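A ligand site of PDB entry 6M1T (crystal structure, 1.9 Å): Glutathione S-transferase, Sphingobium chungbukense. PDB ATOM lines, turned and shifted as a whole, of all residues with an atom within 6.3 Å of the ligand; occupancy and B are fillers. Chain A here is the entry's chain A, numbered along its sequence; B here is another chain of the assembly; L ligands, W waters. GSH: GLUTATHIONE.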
ATOM      1  N   SER A   6     -25.558  18.463   9.337  1.00  0.00           N
ATOM      2  CA  SER A   6     -24.593  19.165   8.468  1.00  0.00           C
ATOM      3  C   SER A   6     -25.398  20.108   7.576  1.00  0.00           C
ATOM      4  O   SER A   6     -26.363  19.695   6.943  1.00  0.00           O
ATOM      5  CB  SER A   6     -23.783  18.145   7.702  1.00  0.00           C
ATOM      6  OG  SER A   6     -22.835  18.825   6.894  1.00  0.00           O
ATOM      7  N   ALA A   9     -27.690  19.327   4.322  1.00  0.00           N
ATOM      8  CA  ALA A   9     -27.720  17.861   4.117  1.00  0.00           C
ATOM      9  C   ALA A   9     -29.130  17.360   4.396  1.00  0.00           C
ATOM     10  O   ALA A   9     -30.014  18.214   4.711  1.00  0.00           O
ATOM     11  CB  ALA A   9     -26.673  17.194   4.977  1.00  0.00           C
ATOM     12  N   CYS A  10     -29.379  16.041   4.295  1.00  0.00           N
ATOM     13  CA  CYS A  10     -30.754  15.514   4.478  1.00  0.00           C
ATOM     14  C   CYS A  10     -31.196  15.712   5.936  1.00  0.00           C
ATOM     15  O   CYS A  10     -32.447  15.652   6.204  1.00  0.00           O
ATOM     16  CB  CYS A  10     -30.864  14.075   4.012  1.00  0.00           C
ATOM     17  SG  CYS A  10     -29.707  13.092   4.980  1.00  0.00           S
ATOM     18  N   SER A  11     -30.263  16.020   6.862  1.00  0.00           N
ATOM     19  CA  SER A  11     -30.575  16.426   8.263  1.00  0.00           C
ATOM     20  C   SER A  11     -31.428  17.700   8.364  1.00  0.00           C
ATOM     21  O   SER A  11     -32.077  17.909   9.443  1.00  0.00           O
ATOM     22  CB  SER A  11     -29.306  16.559   9.103  1.00  0.00           C
ATOM     23  OG  SER A  11     -28.322  17.323   8.450  1.00  0.00           O
ATOM     24  N   LEU A  32     -18.444  16.242   8.483  1.00  0.00           N
ATOM     25  CA  LEU A  32     -18.693  14.881   7.906  1.00  0.00           C
ATOM     26  C   LEU A  32     -17.354  14.262   7.440  1.00  0.00           C
ATOM     27  O   LEU A  32     -17.258  13.014   7.372  1.00  0.00           O
ATOM     28  CB  LEU A  32     -19.722  15.042   6.778  1.00  0.00           C
ATOM     29  CG  LEU A  32     -21.156  15.271   7.277  1.00  0.00           C
ATOM     30  CD1 LEU A  32     -22.098  15.320   6.092  1.00  0.00           C
ATOM     31  CD2 LEU A  32     -21.569  14.199   8.307  1.00  0.00           C
ATOM     32  N   ARG A  35     -15.758  13.267  10.892  1.00  0.00           N
ATOM     33  CA  ARG A  35     -16.725  12.649  11.815  1.00  0.00           C
ATOM     34  C   ARG A  35     -16.542  13.214  13.234  1.00  0.00           C
ATOM     35  O   ARG A  35     -16.642  12.433  14.205  1.00  0.00           O
ATOM     36  CB  ARG A  35     -16.617  11.115  11.880  1.00  0.00           C
ATOM     37  CG  ARG A  35     -17.366  10.390  10.764  1.00  0.00           C
ATOM     38  CD  ARG A  35     -16.725  10.564   9.408  1.00  0.00           C
ATOM     39  NE  ARG A  35     -17.319   9.852   8.295  1.00  0.00           N
ATOM     40  CZ  ARG A  35     -16.692   8.955   7.522  1.00  0.00           C
ATOM     41  NH1 ARG A  35     -15.455   8.561   7.778  1.00  0.00           N
ATOM     42  NH2 ARG A  35     -17.337   8.426   6.490  1.00  0.00           N
ATOM     43  N   SER A  49     -22.098   4.756  11.833  1.00  0.00           N
ATOM     44  CA  SER A  49     -21.948   4.890  10.375  1.00  0.00           C
ATOM     45  C   SER A  49     -21.387   6.269  10.037  1.00  0.00           C
ATOM     46  O   SER A  49     -20.929   6.469   8.947  1.00  0.00           O
ATOM     47  CB  SER A  49     -23.261   4.651   9.699  1.00  0.00           C
ATOM     48  OG  SER A  49     -24.104   5.766   9.878  1.00  0.00           O
ATOM     49  N   GLY A  50     -21.421   7.213  10.963  1.00  0.00           N
ATOM     50  CA  GLY A  50     -20.869   8.546  10.718  1.00  0.00           C
ATOM     51  C   GLY A  50     -21.838   9.451   9.941  1.00  0.00           C
ATOM     52  O   GLY A  50     -21.413  10.520   9.489  1.00  0.00           O
ATOM     53  N   LYS A  51     -23.083   9.065   9.759  1.00  0.00           N
ATOM     54  CA  LYS A  51     -23.990   9.848   8.873  1.00  0.00           C
ATOM     55  C   LYS A  51     -24.961  10.716   9.697  1.00  0.00           C
ATOM     56  O   LYS A  51     -25.351  10.352  10.836  1.00  0.00           O
ATOM     57  CB  LYS A  51     -24.772   8.918   7.957  1.00  0.00           C
ATOM     58  CG  LYS A  51     -23.935   8.119   6.978  1.00  0.00           C
ATOM     59  CD  LYS A  51     -24.739   7.068   6.282  1.00  0.00           C
ATOM     60  CE  LYS A  51     -23.975   6.404   5.170  1.00  0.00           C
ATOM     61  NZ  LYS A  51     -24.179   7.182   3.939  1.00  0.00           N
ATOM     62  N   VAL A  52     -25.391  11.816   9.078  1.00  0.00           N
ATOM     63  CA  VAL A  52     -26.465  12.688   9.637  1.00  0.00           C
ATOM     64  C   VAL A  52     -27.711  12.402   8.812  1.00  0.00           C
ATOM     65  O   VAL A  52     -27.590  12.044   7.659  1.00  0.00           O
ATOM     66  CB  VAL A  52     -26.071  14.177   9.662  1.00  0.00           C
ATOM     67  CG1 VAL A  52     -25.006  14.427  10.710  1.00  0.00           C
ATOM     68  CG2 VAL A  52     -25.682  14.753   8.294  1.00  0.00           C
ATOM     69  N   PRO A  53     -28.931  12.536   9.370  1.00  0.00           N
ATOM     70  CA  PRO A  53     -29.121  12.957  10.774  1.00  0.00           C
ATOM     71  C   PRO A  53     -28.954  11.842  11.803  1.00  0.00           C
ATOM     72  O   PRO A  53     -29.130  10.681  11.459  1.00  0.00           O
ATOM     73  CB  PRO A  53     -30.603  13.386  10.835  1.00  0.00           C
ATOM     74  CG  PRO A  53     -31.252  12.528   9.745  1.00  0.00           C
ATOM     75  CD  PRO A  53     -30.210  12.351   8.665  1.00  0.00           C
ATOM     76  N   THR A  64     -31.459   6.744  14.337  1.00  0.00           N
ATOM     77  CA  THR A  64     -30.897   7.075  13.009  1.00  0.00           C
ATOM     78  C   THR A  64     -31.928   6.766  11.925  1.00  0.00           C
ATOM     79  O   THR A  64     -32.919   6.075  12.232  1.00  0.00           O
ATOM     80  CB  THR A  64     -29.580   6.341  12.720  1.00  0.00           C
ATOM     81  OG1 THR A  64     -29.862   4.944  12.779  1.00  0.00           O
ATOM     82  CG2 THR A  64     -28.468   6.650  13.690  1.00  0.00           C
ATOM     83  N   GLU A  65     -31.662   7.245  10.714  1.00  0.00           N
ATOM     84  CA  GLU A  65     -32.514   7.080   9.509  1.00  0.00           C
ATOM     85  C   GLU A  65     -33.644   8.098   9.552  1.00  0.00           C
ATOM     86  O   GLU A  65     -34.524   8.032  10.450  1.00  0.00           O
ATOM     87  CB  GLU A  65     -33.070   5.643   9.382  1.00  0.00           C
ATOM     88  CG  GLU A  65     -32.003   4.562   9.352  1.00  0.00           C
ATOM     89  CD  GLU A  65     -31.136   4.537   8.120  1.00  0.00           C
ATOM     90  OE1 GLU A  65     -29.965   4.112   8.250  1.00  0.00           O
ATOM     91  OE2 GLU A  65     -31.637   4.916   7.005  1.00  0.00           O
ATOM     92  N   ASN A  66     -33.671   8.945   8.531  1.00  0.00           N
ATOM     93  CA  ASN A  66     -34.690  10.012   8.346  1.00  0.00           C
ATOM     94  C   ASN A  66     -36.092   9.472   8.542  1.00  0.00           C
ATOM     95  O   ASN A  66     -36.882  10.060   9.293  1.00  0.00           O
ATOM     96  CB  ASN A  66     -34.484  10.735   7.018  1.00  0.00           C
ATOM     97  CG  ASN A  66     -33.928  12.125   7.267  1.00  0.00           C
ATOM     98  OD1 ASN A  66     -34.273  12.739   8.267  1.00  0.00           O
ATOM     99  ND2 ASN A  66     -33.068  12.589   6.408  1.00  0.00           N
ATOM    100  N   PRO A  67     -36.485   8.373   7.870  1.00  0.00           N
ATOM    101  CA  PRO A  67     -37.857   7.875   8.007  1.00  0.00           C
ATOM    102  C   PRO A  67     -38.293   7.620   9.461  1.00  0.00           C
ATOM    103  O   PRO A  67     -39.435   8.002   9.853  1.00  0.00           O
ATOM    104  CB  PRO A  67     -37.812   6.599   7.143  1.00  0.00           C
ATOM    105  CG  PRO A  67     -36.804   6.893   6.084  1.00  0.00           C
ATOM    106  CD  PRO A  67     -35.705   7.652   6.830  1.00  0.00           C
ATOM    107  N   ILE A  69     -36.706   8.942  12.269  1.00  0.00           N
ATOM    108  CA  ILE A  69     -36.542  10.221  13.006  1.00  0.00           C
ATOM    109  C   ILE A  69     -37.750  11.090  12.750  1.00  0.00           C
ATOM    110  O   ILE A  69     -38.284  11.617  13.702  1.00  0.00           O
ATOM    111  CB  ILE A  69     -35.215  10.908  12.630  1.00  0.00           C
ATOM    112  CG1 ILE A  69     -34.052  10.061  13.174  1.00  0.00           C
ATOM    113  CG2 ILE A  69     -35.169  12.340  13.144  1.00  0.00           C
ATOM    114  CD1 ILE A  69     -32.681  10.439  12.678  1.00  0.00           C
ATOM    115  N   GLY A 102     -35.897   8.124   0.756  1.00  0.00           N
ATOM    116  CA  GLY A 102     -34.621   7.661   1.352  1.00  0.00           C
ATOM    117  C   GLY A 102     -33.896   6.622   0.497  1.00  0.00           C
ATOM    118  O   GLY A 102     -32.658   6.695   0.380  1.00  0.00           O
ATOM    119  N   HIS A 106     -32.976   9.969  -2.863  1.00  0.00           N
ATOM    120  CA  HIS A 106     -31.702  10.346  -2.182  1.00  0.00           C
ATOM    121  C   HIS A 106     -30.572   9.671  -2.929  1.00  0.00           C
ATOM    122  O   HIS A 106     -29.567  10.348  -3.208  1.00  0.00           O
ATOM    123  CB  HIS A 106     -31.747  10.000  -0.667  1.00  0.00           C
ATOM    124  CG  HIS A 106     -30.567  10.468   0.147  1.00  0.00           C
ATOM    125  ND1 HIS A 106     -29.266  10.386  -0.283  1.00  0.00           N
ATOM    126  CD2 HIS A 106     -30.483  10.949   1.404  1.00  0.00           C
ATOM    127  CE1 HIS A 106     -28.445  10.858   0.643  1.00  0.00           C
ATOM    128  NE2 HIS A 106     -29.166  11.212   1.684  1.00  0.00           N
ATOM    129  N   LYS A 107     -30.670   8.361  -3.127  1.00  0.00           N
ATOM    130  CA  LYS A 107     -29.528   7.520  -3.560  1.00  0.00           C
ATOM    131  C   LYS A 107     -29.232   7.841  -5.042  1.00  0.00           C
ATOM    132  O   LYS A 107     -28.035   7.801  -5.395  1.00  0.00           O
ATOM    133  CB  LYS A 107     -29.772   6.033  -3.234  1.00  0.00           C
ATOM    134  CG  LYS A 107     -29.862   5.696  -1.739  1.00  0.00           C
ATOM    135  CD  LYS A 107     -28.841   6.416  -0.864  1.00  0.00           C
ATOM    136  CE  LYS A 107     -28.455   5.744   0.425  1.00  0.00           C
ATOM    137  NZ  LYS A 107     -27.147   5.040   0.290  1.00  0.00           N
ATOM    138  N   TYR A 157     -39.327  16.327   3.819  1.00  0.00           N
ATOM    139  CA  TYR A 157     -38.197  15.499   3.309  1.00  0.00           C
ATOM    140  C   TYR A 157     -37.995  15.734   1.808  1.00  0.00           C
ATOM    141  O   TYR A 157     -36.866  16.006   1.375  1.00  0.00           O
ATOM    142  CB  TYR A 157     -38.547  14.071   3.635  1.00  0.00           C
ATOM    143  CG  TYR A 157     -37.429  13.057   3.585  1.00  0.00           C
ATOM    144  CD1 TYR A 157     -36.090  13.401   3.712  1.00  0.00           C
ATOM    145  CD2 TYR A 157     -37.770  11.721   3.531  1.00  0.00           C
ATOM    146  CE1 TYR A 157     -35.102  12.417   3.701  1.00  0.00           C
ATOM    147  CE2 TYR A 157     -36.812  10.729   3.554  1.00  0.00           C
ATOM    148  CZ  TYR A 157     -35.483  11.073   3.653  1.00  0.00           C
ATOM    149  OH  TYR A 157     -34.558  10.061   3.616  1.00  0.00           O
ATOM    150  N   TRP A 164     -31.453  20.125  -3.868  1.00  0.00           N
ATOM    151  CA  TRP A 164     -30.145  19.560  -4.305  1.00  0.00           C
ATOM    152  C   TRP A 164     -29.853  19.691  -5.805  1.00  0.00           C
ATOM    153  O   TRP A 164     -28.722  19.976  -6.158  1.00  0.00           O
ATOM    154  CB  TRP A 164     -30.020  18.100  -3.894  1.00  0.00           C
ATOM    155  CG  TRP A 164     -29.949  17.938  -2.410  1.00  0.00           C
ATOM    156  CD1 TRP A 164     -29.764  18.891  -1.446  1.00  0.00           C
ATOM    157  CD2 TRP A 164     -30.062  16.681  -1.724  1.00  0.00           C
ATOM    158  NE1 TRP A 164     -29.737  18.304  -0.205  1.00  0.00           N
ATOM    159  CE2 TRP A 164     -29.950  16.951  -0.346  1.00  0.00           C
ATOM    160  CE3 TRP A 164     -30.282  15.395  -2.170  1.00  0.00           C
ATOM    161  CZ2 TRP A 164     -30.029  15.937   0.609  1.00  0.00           C
ATOM    162  CZ3 TRP A 164     -30.406  14.390  -1.236  1.00  0.00           C
ATOM    163  CH2 TRP A 164     -30.263  14.667   0.122  1.00  0.00           C
ATOM    164  N   SER B  99     -35.361   0.980   7.382  1.00  0.00           N
ATOM    165  CA  SER B  99     -34.849   2.103   6.538  1.00  0.00           C
ATOM    166  C   SER B  99     -33.376   1.799   6.194  1.00  0.00           C
ATOM    167  O   SER B  99     -32.932   2.020   5.021  1.00  0.00           O
ATOM    168  CB  SER B  99     -35.065   3.541   7.130  1.00  0.00           C
ATOM    169  OG  SER B  99     -33.897   4.157   6.615  1.00  0.00           O
ATOM    170  N   PHE B 100     -32.582   1.373   7.170  1.00  0.00           N
ATOM    171  CA  PHE B 100     -31.164   1.057   6.931  1.00  0.00           C
ATOM    172  C   PHE B 100     -31.035  -0.074   5.902  1.00  0.00           C
ATOM    173  O   PHE B 100     -30.259   0.058   4.898  1.00  0.00           O
ATOM    174  CB  PHE B 100     -30.428   0.682   8.220  1.00  0.00           C
ATOM    175  CG  PHE B 100     -29.054   0.144   7.936  1.00  0.00           C
ATOM    176  CD1 PHE B 100     -27.963   1.000   7.810  1.00  0.00           C
ATOM    177  CD2 PHE B 100     -28.859  -1.217   7.790  1.00  0.00           C
ATOM    178  CE1 PHE B 100     -26.692   0.494   7.623  1.00  0.00           C
ATOM    179  CE2 PHE B 100     -27.585  -1.719   7.525  1.00  0.00           C
ATOM    180  CZ  PHE B 100     -26.506  -0.864   7.434  1.00  0.00           C
ATOM    181  N   SER B 103     -32.410   1.440   2.364  1.00  0.00           N
ATOM    182  CA  SER B 103     -31.687   2.611   1.806  1.00  0.00           C
ATOM    183  C   SER B 103     -30.188   2.347   1.696  1.00  0.00           C
ATOM    184  O   SER B 103     -29.545   3.020   0.885  1.00  0.00           O
ATOM    185  CB  SER B 103     -31.948   3.840   2.648  1.00  0.00           C
ATOM    186  OG  SER B 103     -31.171   3.831   3.865  1.00  0.00           O
ATOM    187  N   GLU B 104     -29.609   1.452   2.507  1.00  0.00           N
ATOM    188  CA  GLU B 104     -28.132   1.342   2.546  1.00  0.00           C
ATOM    189  C   GLU B 104     -27.785  -0.053   2.004  1.00  0.00           C
ATOM    190  O   GLU B 104     -27.034  -0.179   1.037  1.00  0.00           O
ATOM    191  CB  GLU B 104     -27.580   1.598   3.948  1.00  0.00           C
ATOM    192  CG  GLU B 104     -27.965   2.941   4.554  1.00  0.00           C
ATOM    193  CD  GLU B 104     -27.330   4.116   3.839  1.00  0.00           C
ATOM    194  OE1 GLU B 104     -27.681   5.231   4.186  1.00  0.00           O
ATOM    195  OE2 GLU B 104     -26.518   3.929   2.935  1.00  0.00           O
HETATM  196  N1  GSH L   1     -30.253   6.343   4.988  1.00  0.00           N
HETATM  197  CA1 GSH L   1     -29.824   7.498   5.796  1.00  0.00           C
HETATM  198  C1  GSH L   1     -31.048   8.295   6.272  1.00  0.00           C
HETATM  199  O11 GSH L   1     -32.066   8.182   5.586  1.00  0.00           O
HETATM  200  O12 GSH L   1     -30.906   9.000   7.324  1.00  0.00           O
HETATM  201  CB1 GSH L   1     -28.905   8.358   4.926  1.00  0.00           C
HETATM  202  CG1 GSH L   1     -28.112   9.397   5.679  1.00  0.00           C
HETATM  203  CD1 GSH L   1     -27.091  10.044   4.753  1.00  0.00           C
HETATM  204  OE1 GSH L   1     -26.683   9.497   3.712  1.00  0.00           O
HETATM  205  N2  GSH L   1     -26.609  11.204   5.155  1.00  0.00           N
HETATM  206  CA2 GSH L   1     -25.573  11.974   4.489  1.00  0.00           C
HETATM  207  C2  GSH L   1     -24.234  11.846   5.195  1.00  0.00           C
HETATM  208  O2  GSH L   1     -24.165  11.992   6.421  1.00  0.00           O
HETATM  209  CB2 GSH L   1     -25.965  13.448   4.363  1.00  0.00           C
HETATM  210  SG2 GSH L   1     -27.276  13.752   3.146  1.00  0.00           S
HETATM  211  N3  GSH L   1     -23.209  11.491   4.441  1.00  0.00           N
HETATM  212  CA3 GSH L   1     -21.871  11.366   4.955  1.00  0.00           C
HETATM  213  C3  GSH L   1     -21.243  10.013   4.649  1.00  0.00           C
HETATM  214  O31 GSH L   1     -21.987   9.112   4.194  1.00  0.00           O
HETATM  215  O32 GSH L   1     -20.023   9.872   4.896  1.00  0.00           O
HETATM  216  O   HOH W   1     -33.523   5.950   4.854  1.00  0.00           O
HETATM  217  O   HOH W   2     -29.538   8.640   9.591  1.00  0.00           O
HETATM  218  O   HOH W   3     -27.767   5.179   6.990  1.00  0.00           O
HETATM  219  O   HOH W   4     -31.014   7.503   2.292  1.00  0.00           O
HETATM  220  O   HOH W   5     -32.095  10.500   3.779  1.00  0.00           O
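The backbone NH (N) of Val 52 is in hydrogen-bond range of an oxygen (O2) of the ligand. A nitrogen (N2) of the ligand lies within hydrogen-bond range of the backbone carbonyl oxygen (O) of Val 52 (2.8 Å). A nitrogen (N1) of the ligand lies within salt-bridge range of the side-chain carboxylate (OE2) of Glu 65. OG of Ser 103 of chain B is in hydrogen-bond range of N1 of the ligand, at 2.9 Å. The side-chain carboxylate of Glu 104 of chain B lies within salt-bridge range of a nitrogen (N1) of the ligand (2.9 Å). The side-chain amino group (NZ) of Lys 51 lies within salt-bridge range of an oxygen (O31) of the ligand, at 2.9 Å. The backbone NH (N) of Asn 66 sits at hydrogen-bond distance from an oxygen (O12) of the ligand, 3.0 Å away. The backbone NH (N) of Cys 10 lies close to a sulfur (SG2) of the ligand, at 3.3 Å. SG of Cys 10 lies close to SG2 of the ligand, 3.1 Å away. An oxygen (O32) of the ligand lies within salt-bridge range of the guanidinium group (NH2) of Arg 35, at 3.4 Å. NE2 of His 106 sits close to SG2 of the ligand (3.5 Å).
O of Val 52 lies within hydrogen-bond range of SG of Cys 10 (3.6 Å). The side-chain carboxylate of Glu 65 lies within hydrogen-bond range of the side-chain hydroxyl of Ser 99 of chain B, at 2.4 Å. The side-chain hydroxyl of Ser 103 of chain B lies within hydrogen-bond range of the backbone carbonyl oxygen of Ser 99 of chain B (2.8 Å). The backbone carbonyl oxygen (O) of Ser 103 of chain B lies close to the side-chain amino group (NZ) of Lys 107, at 3.2 Å. The side-chain carboxylate (OE2) of Glu 104 of chain B lies within salt-bridge range of the side-chain amino group (NZ) of Lys 107 (2.9 Å). OG of Ser 49 lies close to N of Lys 51 (3.5 Å). ND2 of Asn 66 is in hydrogen-bond range of O of Cys 10 (3.1 Å). NE of Arg 35 sits close to O of Leu 32, at 3.3 Å.
Merely in contact with the ligand: Ala 9, Leu 32, Pro 53, Pro 67 and Tyr 157. Hydrophobic or aromatic side chains that line the ligand: Ala 9, Leu 32, Val 52, Pro 53, Pro 67 and His 106. 14 residues have an atom within 4 Å of the ligand: Ala 9, Cys 10, Leu 32, Arg 35, Lys 51, Val 52, Pro 53, Glu 65, Asn 66, Pro 67, His 106, Tyr 157, Ser 103 of chain B and Glu 104 of chain B.
Water W2 lies within hydrogen-bond range of O12 of the ligand, N of Glu 65 and O of Pro 53. Water W1 lies within hydrogen-bond range of OG of Ser 99 of chain B (2.5 Å), O11 of the ligand (2.8 Å), OE2 of Glu 65 (3.0 Å) and OG of Ser 103 of chain B (3.3 Å). Water W5 lies within hydrogen-bond range of OH of Tyr 157, O11 of the ligand, ND2 of Asn 66 and SG of Cys 10. Water W4 lies within hydrogen-bond range of the backbone carbonyl oxygen (O) of Gly 102 (2.6 Å) and a nitrogen (N1) of the ligand (3.0 Å). Water W3 lies within hydrogen-bond range of OE1 of Glu 65 (2.7 Å), OE1 of Glu 104 of chain B (2.8 Å) and N1 of the ligand (3.4 Å).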
